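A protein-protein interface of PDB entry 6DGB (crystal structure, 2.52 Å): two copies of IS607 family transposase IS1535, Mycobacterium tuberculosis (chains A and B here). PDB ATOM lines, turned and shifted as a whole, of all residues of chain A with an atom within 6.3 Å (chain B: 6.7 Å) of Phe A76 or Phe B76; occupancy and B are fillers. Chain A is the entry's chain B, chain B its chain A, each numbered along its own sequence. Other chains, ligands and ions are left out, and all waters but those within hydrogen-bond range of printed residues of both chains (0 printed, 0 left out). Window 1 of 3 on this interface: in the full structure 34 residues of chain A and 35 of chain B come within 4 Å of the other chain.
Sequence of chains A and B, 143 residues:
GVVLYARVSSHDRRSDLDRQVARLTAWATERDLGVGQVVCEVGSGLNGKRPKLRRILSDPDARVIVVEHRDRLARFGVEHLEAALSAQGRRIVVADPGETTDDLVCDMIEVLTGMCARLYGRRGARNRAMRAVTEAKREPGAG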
ATOM      1  N   GLY A  45      -1.661  -6.706   2.008  1.00  0.00           N
ATOM      2  CA  GLY A  45      -0.253  -6.465   2.316  1.00  0.00           C
ATOM      3  C   GLY A  45       0.282  -5.219   1.628  1.00  0.00           C
ATOM      4  O   GLY A  45       1.475  -4.928   1.713  1.00  0.00           O
ATOM      5  N   LEU A  46      -0.617  -4.482   0.933  1.00  0.00           N
ATOM      6  CA  LEU A  46      -0.342  -3.251   0.185  1.00  0.00           C
ATOM      7  C   LEU A  46      -1.254  -2.120   0.695  1.00  0.00           C
ATOM      8  O   LEU A  46      -1.670  -1.242  -0.064  1.00  0.00           O
ATOM      9  CB  LEU A  46      -0.552  -3.474  -1.329  1.00  0.00           C
ATOM     10  CG  LEU A  46      -0.106  -4.806  -1.930  1.00  0.00           C
ATOM     11  CD1 LEU A  46      -0.829  -5.063  -3.219  1.00  0.00           C
ATOM     12  CD2 LEU A  46       1.403  -4.860  -2.139  1.00  0.00           C
ATOM     13  N   ALA A  74       3.743  -3.834   6.045  1.00  0.00           N
ATOM     14  CA  ALA A  74       3.679  -3.632   4.589  1.00  0.00           C
ATOM     15  C   ALA A  74       4.627  -4.573   3.857  1.00  0.00           C
ATOM     16  O   ALA A  74       5.796  -4.716   4.257  1.00  0.00           O
ATOM     17  CB  ALA A  74       4.020  -2.197   4.227  1.00  0.00           C
ATOM     18  N   ARG A  75       4.131  -5.190   2.760  1.00  0.00           N
ATOM     19  CA  ARG A  75       4.914  -6.068   1.884  1.00  0.00           C
ATOM     20  C   ARG A  75       5.993  -5.226   1.190  1.00  0.00           C
ATOM     21  O   ARG A  75       7.090  -5.740   0.961  1.00  0.00           O
ATOM     22  CB  ARG A  75       4.003  -6.744   0.831  1.00  0.00           C
ATOM     23  CG  ARG A  75       4.643  -7.886   0.038  1.00  0.00           C
ATOM     24  CD  ARG A  75       4.877  -9.169   0.848  1.00  0.00           C
ATOM     25  NE  ARG A  75       3.670  -9.605   1.547  1.00  0.00           N
ATOM     26  CZ  ARG A  75       3.585 -10.688   2.306  1.00  0.00           C
ATOM     27  NH1 ARG A  75       2.446 -10.996   2.902  1.00  0.00           N
ATOM     28  NH2 ARG A  75       4.638 -11.482   2.465  1.00  0.00           N
ATOM     29  N   PHE A  76       5.668  -3.928   0.868  1.00  0.00           N
ATOM     30  CA  PHE A  76       6.550  -2.932   0.222  1.00  0.00           C
ATOM     31  C   PHE A  76       6.472  -1.543   0.887  1.00  0.00           C
ATOM     32  O   PHE A  76       5.391  -1.136   1.342  1.00  0.00           O
ATOM     33  CB  PHE A  76       6.283  -2.787  -1.318  1.00  0.00           C
ATOM     34  CG  PHE A  76       6.262  -4.080  -2.094  1.00  0.00           C
ATOM     35  CD1 PHE A  76       7.437  -4.798  -2.318  1.00  0.00           C
ATOM     36  CD2 PHE A  76       5.063  -4.625  -2.532  1.00  0.00           C
ATOM     37  CE1 PHE A  76       7.407  -6.043  -2.961  1.00  0.00           C
ATOM     38  CE2 PHE A  76       5.034  -5.862  -3.184  1.00  0.00           C
ATOM     39  CZ  PHE A  76       6.209  -6.561  -3.397  1.00  0.00           C
ATOM     40  N   GLY A  77       7.625  -0.855   0.917  1.00  0.00           N
ATOM     41  CA  GLY A  77       7.783   0.513   1.394  1.00  0.00           C
ATOM     42  C   GLY A  77       8.111   0.784   2.846  1.00  0.00           C
ATOM     43  O   GLY A  77       8.193   1.964   3.228  1.00  0.00           O
ATOM     44  N   VAL A  78       8.319  -0.295   3.664  1.00  0.00           N
ATOM     45  CA  VAL A  78       8.581  -0.181   5.108  1.00  0.00           C
ATOM     46  C   VAL A  78       9.772   0.756   5.400  1.00  0.00           C
ATOM     47  O   VAL A  78       9.656   1.601   6.287  1.00  0.00           O
ATOM     48  CB  VAL A  78       8.689  -1.556   5.824  1.00  0.00           C
ATOM     49  CG1 VAL A  78       9.232  -1.420   7.242  1.00  0.00           C
ATOM     50  CG2 VAL A  78       7.331  -2.245   5.858  1.00  0.00           C
ATOM     51  N   GLU A  79      10.856   0.654   4.623  1.00  0.00           N
ATOM     52  CA  GLU A  79      12.026   1.513   4.791  1.00  0.00           C
ATOM     53  C   GLU A  79      11.690   3.024   4.702  1.00  0.00           C
ATOM     54  O   GLU A  79      12.284   3.830   5.435  1.00  0.00           O
ATOM     55  CB  GLU A  79      13.157   1.122   3.818  1.00  0.00           C
ATOM     56  CG  GLU A  79      12.759   1.034   2.344  1.00  0.00           C
ATOM     57  CD  GLU A  79      13.917   1.047   1.355  1.00  0.00           C
ATOM     58  OE1 GLU A  79      14.877   0.267   1.554  1.00  0.00           O
ATOM     59  OE2 GLU A  79      13.855   1.822   0.370  1.00  0.00           O
ATOM     60  N   LEU A  81       8.471   4.341   5.291  1.00  0.00           N
ATOM     61  CA  LEU A  81       7.630   4.618   6.452  1.00  0.00           C
ATOM     62  C   LEU A  81       8.536   4.927   7.650  1.00  0.00           C
ATOM     63  O   LEU A  81       8.308   5.929   8.332  1.00  0.00           O
ATOM     64  CB  LEU A  81       6.739   3.409   6.808  1.00  0.00           C
ATOM     65  CG  LEU A  81       5.407   3.278   6.103  1.00  0.00           C
ATOM     66  CD1 LEU A  81       4.674   2.048   6.597  1.00  0.00           C
ATOM     67  CD2 LEU A  81       4.538   4.486   6.353  1.00  0.00           C
ATOM     68  N   GLU A 110      -2.771 -10.654  -5.881  1.00  0.00           N
ATOM     69  CA  GLU A 110      -3.277  -9.333  -5.479  1.00  0.00           C
ATOM     70  C   GLU A 110      -2.580  -8.201  -6.232  1.00  0.00           C
ATOM     71  O   GLU A 110      -3.214  -7.193  -6.551  1.00  0.00           O
ATOM     72  CB  GLU A 110      -3.005  -9.170  -3.966  1.00  0.00           C
ATOM     73  CG  GLU A 110      -3.736  -8.050  -3.233  1.00  0.00           C
ATOM     74  CD  GLU A 110      -3.420  -7.979  -1.745  1.00  0.00           C
ATOM     75  OE1 GLU A 110      -3.940  -8.820  -0.976  1.00  0.00           O
ATOM     76  OE2 GLU A 110      -2.639  -7.083  -1.350  1.00  0.00           O
ATOM     77  N   VAL A 111      -1.269  -8.378  -6.491  1.00  0.00           N
ATOM     78  CA  VAL A 111      -0.344  -7.460  -7.157  1.00  0.00           C
ATOM     79  C   VAL A 111      -0.463  -7.584  -8.662  1.00  0.00           C
ATOM     80  O   VAL A 111      -0.656  -6.575  -9.342  1.00  0.00           O
ATOM     81  CB  VAL A 111       1.096  -7.721  -6.663  1.00  0.00           C
ATOM     82  CG1 VAL A 111       2.140  -7.215  -7.650  1.00  0.00           C
ATOM     83  CG2 VAL A 111       1.299  -7.110  -5.292  1.00  0.00           C
ATOM     84  N   MET A 115      -1.794  -4.851 -11.544  1.00  0.00           N
ATOM     85  CA  MET A 115      -0.803  -4.519 -12.549  1.00  0.00           C
ATOM     86  C   MET A 115      -1.275  -4.953 -13.934  1.00  0.00           C
ATOM     87  O   MET A 115      -1.011  -4.247 -14.896  1.00  0.00           O
ATOM     88  CB  MET A 115       0.558  -5.106 -12.154  1.00  0.00           C
ATOM     89  CG  MET A 115       1.181  -4.435 -10.911  1.00  0.00           C
ATOM     90  SD  MET A 115       2.951  -4.827 -10.744  1.00  0.00           S
ATOM     91  CE  MET A 115       3.506  -3.426  -9.808  1.00  0.00           C
ATOM     92  N   ARG A 118      -4.223  -2.485 -15.033  1.00  0.00           N
ATOM     93  CA  ARG A 118      -3.659  -1.225 -15.514  1.00  0.00           C
ATOM     94  C   ARG A 118      -3.084  -1.414 -16.925  1.00  0.00           C
ATOM     95  O   ARG A 118      -3.227  -0.535 -17.774  1.00  0.00           O
ATOM     96  CB  ARG A 118      -2.576  -0.704 -14.548  1.00  0.00           C
ATOM     97  CG  ARG A 118      -3.085  -0.107 -13.224  1.00  0.00           C
ATOM     98  CD  ARG A 118      -1.996  -0.163 -12.151  1.00  0.00           C
ATOM     99  NE  ARG A 118      -2.528  -0.164 -10.779  1.00  0.00           N
ATOM    100  CZ  ARG A 118      -1.918  -0.710  -9.725  1.00  0.00           C
ATOM    101  NH1 ARG A 118      -0.746  -1.324  -9.866  1.00  0.00           N
ATOM    102  NH2 ARG A 118      -2.482  -0.656  -8.523  1.00  0.00           N
ATOM    103  N   GLY B  45      10.344   1.242  -7.985  1.00  0.00           N
ATOM    104  CA  GLY B  45       9.059   1.793  -7.572  1.00  0.00           C
ATOM    105  C   GLY B  45       8.534   1.107  -6.327  1.00  0.00           C
ATOM    106  O   GLY B  45       7.476   1.471  -5.814  1.00  0.00           O
ATOM    107  N   LEU B  46       9.277   0.097  -5.834  1.00  0.00           N
ATOM    108  CA  LEU B  46       8.908  -0.734  -4.684  1.00  0.00           C
ATOM    109  C   LEU B  46       9.939  -0.676  -3.544  1.00  0.00           C
ATOM    110  O   LEU B  46      10.686  -1.624  -3.312  1.00  0.00           O
ATOM    111  CB  LEU B  46       8.687  -2.171  -5.172  1.00  0.00           C
ATOM    112  CG  LEU B  46       7.519  -2.338  -6.123  1.00  0.00           C
ATOM    113  CD1 LEU B  46       7.975  -2.767  -7.474  1.00  0.00           C
ATOM    114  CD2 LEU B  46       6.565  -3.301  -5.600  1.00  0.00           C
ATOM    115  N   ASP B  71       2.465   7.086  -8.168  1.00  0.00           N
ATOM    116  CA  ASP B  71       3.361   5.943  -8.389  1.00  0.00           C
ATOM    117  C   ASP B  71       4.853   6.285  -8.469  1.00  0.00           C
ATOM    118  O   ASP B  71       5.682   5.371  -8.410  1.00  0.00           O
ATOM    119  CB  ASP B  71       2.937   5.127  -9.619  1.00  0.00           C
ATOM    120  CG  ASP B  71       2.861   5.931 -10.897  1.00  0.00           C
ATOM    121  OD1 ASP B  71       1.765   6.467 -11.195  1.00  0.00           O
ATOM    122  OD2 ASP B  71       3.887   6.000 -11.618  1.00  0.00           O
ATOM    123  N   LEU B  73       6.393   8.262  -6.287  1.00  0.00           N
ATOM    124  CA  LEU B  73       6.834   8.264  -4.907  1.00  0.00           C
ATOM    125  C   LEU B  73       6.921   6.822  -4.440  1.00  0.00           C
ATOM    126  O   LEU B  73       7.819   6.506  -3.684  1.00  0.00           O
ATOM    127  CB  LEU B  73       5.869   9.059  -4.017  1.00  0.00           C
ATOM    128  CG  LEU B  73       6.496   9.577  -2.733  1.00  0.00           C
ATOM    129  CD1 LEU B  73       7.079  10.945  -2.933  1.00  0.00           C
ATOM    130  CD2 LEU B  73       5.499   9.642  -1.648  1.00  0.00           C
ATOM    131  N   ALA B  74       5.972   5.959  -4.873  1.00  0.00           N
ATOM    132  CA  ALA B  74       5.866   4.516  -4.572  1.00  0.00           C
ATOM    133  C   ALA B  74       4.708   3.869  -5.338  1.00  0.00           C
ATOM    134  O   ALA B  74       3.619   4.444  -5.418  1.00  0.00           O
ATOM    135  CB  ALA B  74       5.686   4.280  -3.073  1.00  0.00           C
ATOM    136  N   ARG B  75       4.946   2.668  -5.898  1.00  0.00           N
ATOM    137  CA  ARG B  75       3.932   1.858  -6.598  1.00  0.00           C
ATOM    138  C   ARG B  75       2.905   1.370  -5.563  1.00  0.00           C
ATOM    139  O   ARG B  75       1.727   1.253  -5.905  1.00  0.00           O
ATOM    140  CB  ARG B  75       4.592   0.644  -7.279  1.00  0.00           C
ATOM    141  CG  ARG B  75       3.699  -0.114  -8.271  1.00  0.00           C
ATOM    142  CD  ARG B  75       3.468   0.621  -9.599  1.00  0.00           C
ATOM    143  NE  ARG B  75       4.730   1.071 -10.186  1.00  0.00           N
ATOM    144  CZ  ARG B  75       4.864   1.714 -11.339  1.00  0.00           C
ATOM    145  NH1 ARG B  75       3.803   1.983 -12.087  1.00  0.00           N
ATOM    146  NH2 ARG B  75       6.061   2.102 -11.749  1.00  0.00           N
ATOM    147  N   PHE B  76       3.374   1.091  -4.299  1.00  0.00           N
ATOM    148  CA  PHE B  76       2.575   0.651  -3.135  1.00  0.00           C
ATOM    149  C   PHE B  76       2.980   1.391  -1.839  1.00  0.00           C
ATOM    150  O   PHE B  76       4.165   1.728  -1.647  1.00  0.00           O
ATOM    151  CB  PHE B  76       2.640  -0.893  -2.902  1.00  0.00           C
ATOM    152  CG  PHE B  76       2.374  -1.746  -4.122  1.00  0.00           C
ATOM    153  CD1 PHE B  76       1.091  -1.858  -4.650  1.00  0.00           C
ATOM    154  CD2 PHE B  76       3.416  -2.391  -4.782  1.00  0.00           C
ATOM    155  CE1 PHE B  76       0.860  -2.588  -5.828  1.00  0.00           C
ATOM    156  CE2 PHE B  76       3.182  -3.130  -5.951  1.00  0.00           C
ATOM    157  CZ  PHE B  76       1.908  -3.219  -6.466  1.00  0.00           C
ATOM    158  N   GLY B  77       1.979   1.621  -0.983  1.00  0.00           N
ATOM    159  CA  GLY B  77       2.121   2.209   0.352  1.00  0.00           C
ATOM    160  C   GLY B  77       1.999   3.709   0.539  1.00  0.00           C
ATOM    161  O   GLY B  77       2.124   4.181   1.677  1.00  0.00           O
ATOM    162  N   VAL B  78       1.732   4.470  -0.561  1.00  0.00           N
ATOM    163  CA  VAL B  78       1.647   5.946  -0.543  1.00  0.00           C
ATOM    164  C   VAL B  78       0.646   6.450   0.506  1.00  0.00           C
ATOM    165  O   VAL B  78       0.978   7.372   1.251  1.00  0.00           O
ATOM    166  CB  VAL B  78       1.424   6.565  -1.944  1.00  0.00           C
ATOM    167  CG1 VAL B  78       1.069   8.042  -1.859  1.00  0.00           C
ATOM    168  CG2 VAL B  78       2.651   6.369  -2.807  1.00  0.00           C
ATOM    169  N   GLU B  79      -0.524   5.809   0.610  1.00  0.00           N
ATOM    170  CA  GLU B  79      -1.540   6.174   1.599  1.00  0.00           C
ATOM    171  C   GLU B  79      -1.004   6.146   3.056  1.00  0.00           C
ATOM    172  O   GLU B  79      -1.384   7.005   3.868  1.00  0.00           O
ATOM    173  CB  GLU B  79      -2.814   5.321   1.434  1.00  0.00           C
ATOM    174  CG  GLU B  79      -2.588   3.810   1.401  1.00  0.00           C
ATOM    175  CD  GLU B  79      -3.818   2.942   1.623  1.00  0.00           C
ATOM    176  OE1 GLU B  79      -4.875   3.222   1.009  1.00  0.00           O
ATOM    177  OE2 GLU B  79      -3.710   1.956   2.388  1.00  0.00           O
ATOM    178  N   HIS B  80      -0.070   5.194   3.348  1.00  0.00           N
ATOM    179  CA  HIS B  80       0.564   5.016   4.662  1.00  0.00           C
ATOM    180  C   HIS B  80       1.634   6.058   4.926  1.00  0.00           C
ATOM    181  O   HIS B  80       1.750   6.533   6.055  1.00  0.00           O
ATOM    182  CB  HIS B  80       1.089   3.581   4.845  1.00  0.00           C
ATOM    183  CG  HIS B  80       0.018   2.537   4.702  1.00  0.00           C
ATOM    184  ND1 HIS B  80      -1.124   2.559   5.491  1.00  0.00           N
ATOM    185  CD2 HIS B  80      -0.071   1.503   3.832  1.00  0.00           C
ATOM    186  CE1 HIS B  80      -1.860   1.536   5.085  1.00  0.00           C
ATOM    187  NE2 HIS B  80      -1.277   0.884   4.074  1.00  0.00           N
ATOM    188  N   LEU B  81       2.410   6.432   3.875  1.00  0.00           N
ATOM    189  CA  LEU B  81       3.415   7.495   3.945  1.00  0.00           C
ATOM    190  C   LEU B  81       2.706   8.808   4.265  1.00  0.00           C
ATOM    191  O   LEU B  81       3.152   9.519   5.168  1.00  0.00           O
ATOM    192  CB  LEU B  81       4.161   7.653   2.619  1.00  0.00           C
ATOM    193  CG  LEU B  81       5.363   6.755   2.370  1.00  0.00           C
ATOM    194  CD1 LEU B  81       5.980   7.068   1.019  1.00  0.00           C
ATOM    195  CD2 LEU B  81       6.411   6.918   3.449  1.00  0.00           C
ATOM    196  N   LEU B 104       5.618  -0.089 -15.174  1.00  0.00           N
ATOM    197  CA  LEU B 104       4.762  -1.120 -14.576  1.00  0.00           C
ATOM    198  C   LEU B 104       5.148  -2.579 -14.876  1.00  0.00           C
ATOM    199  O   LEU B 104       5.190  -3.390 -13.953  1.00  0.00           O
ATOM    200  CB  LEU B 104       3.314  -0.838 -15.002  1.00  0.00           C
ATOM    201  CG  LEU B 104       2.192  -1.564 -14.313  1.00  0.00           C
ATOM    202  CD1 LEU B 104       2.170  -1.271 -12.826  1.00  0.00           C
ATOM    203  CD2 LEU B 104       0.888  -1.151 -14.918  1.00  0.00           C
ATOM    204  N   ASP B 107       8.172  -3.390 -13.262  1.00  0.00           N
ATOM    205  CA  ASP B 107       7.851  -3.486 -11.833  1.00  0.00           C
ATOM    206  C   ASP B 107       7.169  -4.819 -11.534  1.00  0.00           C
ATOM    207  O   ASP B 107       7.309  -5.330 -10.425  1.00  0.00           O
ATOM    208  CB  ASP B 107       7.045  -2.261 -11.322  1.00  0.00           C
ATOM    209  CG  ASP B 107       7.877  -1.011 -10.984  1.00  0.00           C
ATOM    210  OD1 ASP B 107       9.108  -1.002 -11.262  1.00  0.00           O
ATOM    211  OD2 ASP B 107       7.305  -0.042 -10.468  1.00  0.00           O
ATOM    212  N   GLU B 110      10.291  -7.220 -11.266  1.00  0.00           N
ATOM    213  CA  GLU B 110      11.026  -7.096  -9.993  1.00  0.00           C
ATOM    214  C   GLU B 110      10.211  -7.598  -8.783  1.00  0.00           C
ATOM    215  O   GLU B 110      10.812  -8.121  -7.843  1.00  0.00           O
ATOM    216  CB  GLU B 110      11.624  -5.696  -9.749  1.00  0.00           C
ATOM    217  CG  GLU B 110      10.648  -4.588  -9.361  1.00  0.00           C
ATOM    218  CD  GLU B 110      11.121  -3.157  -9.592  1.00  0.00           C
ATOM    219  OE1 GLU B 110      11.476  -2.814 -10.745  1.00  0.00           O
ATOM    220  OE2 GLU B 110      11.071  -2.357  -8.631  1.00  0.00           O
ATOM    221  N   VAL B 111       8.859  -7.527  -8.848  1.00  0.00           N
ATOM    222  CA  VAL B 111       7.947  -8.041  -7.813  1.00  0.00           C
ATOM    223  C   VAL B 111       7.995  -9.565  -7.819  1.00  0.00           C
ATOM    224  O   VAL B 111       8.254 -10.173  -6.778  1.00  0.00           O
ATOM    225  CB  VAL B 111       6.487  -7.506  -7.991  1.00  0.00           C
ATOM    226  CG1 VAL B 111       5.453  -8.414  -7.327  1.00  0.00           C
ATOM    227  CG2 VAL B 111       6.346  -6.093  -7.458  1.00  0.00           C
ATOM    228  N   MET B 115       9.492 -12.260  -4.983  1.00  0.00           N
ATOM    229  CA  MET B 115       8.482 -13.153  -4.445  1.00  0.00           C
ATOM    230  C   MET B 115       8.806 -14.604  -4.798  1.00  0.00           C
ATOM    231  O   MET B 115       8.564 -15.477  -3.973  1.00  0.00           O
ATOM    232  CB  MET B 115       7.090 -12.720  -4.901  1.00  0.00           C
ATOM    233  CG  MET B 115       6.632 -11.378  -4.280  1.00  0.00           C
ATOM    234  SD  MET B 115       4.837 -11.074  -4.429  1.00  0.00           S
ATOM    235  CE  MET B 115       4.582  -9.912  -3.121  1.00  0.00           C
ATOM    236  N   ARG B 118      11.942 -15.697  -2.559  1.00  0.00           N
ATOM    237  CA  ARG B 118      11.465 -16.034  -1.209  1.00  0.00           C
ATOM    238  C   ARG B 118      10.786 -17.403  -1.200  1.00  0.00           C
ATOM    239  O   ARG B 118      10.994 -18.185  -0.271  1.00  0.00           O
ATOM    240  CB  ARG B 118      10.509 -14.943  -0.665  1.00  0.00           C
ATOM    241  CG  ARG B 118      11.171 -13.615  -0.261  1.00  0.00           C
ATOM    242  CD  ARG B 118      10.179 -12.454  -0.317  1.00  0.00           C
ATOM    243  NE  ARG B 118      10.829 -11.148  -0.499  1.00  0.00           N
ATOM    244  CZ  ARG B 118      10.263 -10.089  -1.083  1.00  0.00           C
ATOM    245  NH1 ARG B 118       9.025 -10.167  -1.561  1.00  0.00           N
ATOM    246  NH2 ARG B 118      10.932  -8.947  -1.196  1.00  0.00           N
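The backbone NH of Arg B75 lies within hydrogen-bond range of the backbone carbonyl oxygen of Gly B45. The guanidinium group of Arg B75 lies within salt-bridge range of the side-chain carboxylate of Asp B107, at 2.8 Å. NE2 of His B80 lies within hydrogen-bond range of OE2 of Glu B79 (3.1 Å). The backbone carbonyl oxygen of Gly A45 sits at hydrogen-bond distance from the backbone NH of Arg A75 (2.9 Å).
Of the 13 printed residues of chain A, 7 touch a printed residue of chain B. Along chain A the printed residues that touch a printed residue of chain B span positions 46 to 118. Of the 18 printed residues of chain B, 8 touch a printed residue of chain A. Along chain B the printed residues that touch a printed residue of chain A span positions 46 to 115.
Among the printed residues, pairs that only touch across the chains: Leu A46 with Phe B76, Arg A75 with Met B115, Phe A76 with Leu B46, Phe A76 with Phe B76, Phe A76 with Met B115, Leu A81 with His B80, Leu A81 with Leu B81, Val A111 with Val B111, Met A115 with Arg B75, Met A115 with Phe B76, Met A115 with Leu B104 and Arg A118 with Leu B104.
Of chain B, only Leu B46 (3.6 Å), Phe B76 (3.6 Å) and Met B115 (3.7 Å) come within 4 Å of Phe A76. Of chain A, only Leu A46 (3.8 Å), Phe A76 (3.6 Å) and Met A115 (3.7 Å) come within 4 Å of Phe B76. Of the printed residues of chain B, Arg A75 touches Met B115 (3.8 Å). Printed residues of chain A within 4 Å of His B80: Leu A81 (3.5 Å). Of the printed residues of chain A, Leu B104 touches Met A115 and Arg A118. Of the printed residues of chain A, Leu B46 touches Phe A76 (3.6 Å). Glu A110 touches none of the printed residues of chain B. Ala A74 touches none of the printed residues of chain B. The nearest residue of chain A that does not touch Phe B76 is Val A111 (4.1 Å).
Leu A46 touches Phe B76, and with the chains exchanged Phe A76 touches Leu B46. Phe A76 touches its own counterpart, Phe B76. Leu A81 touches its own counterpart, Leu B81. Val A111 touches its own counterpart, Val B111. Positions printed for both chains: 45, 46, 74, 75, 76, 77, 78, 79, 81, 110, 111, 115 and 118.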
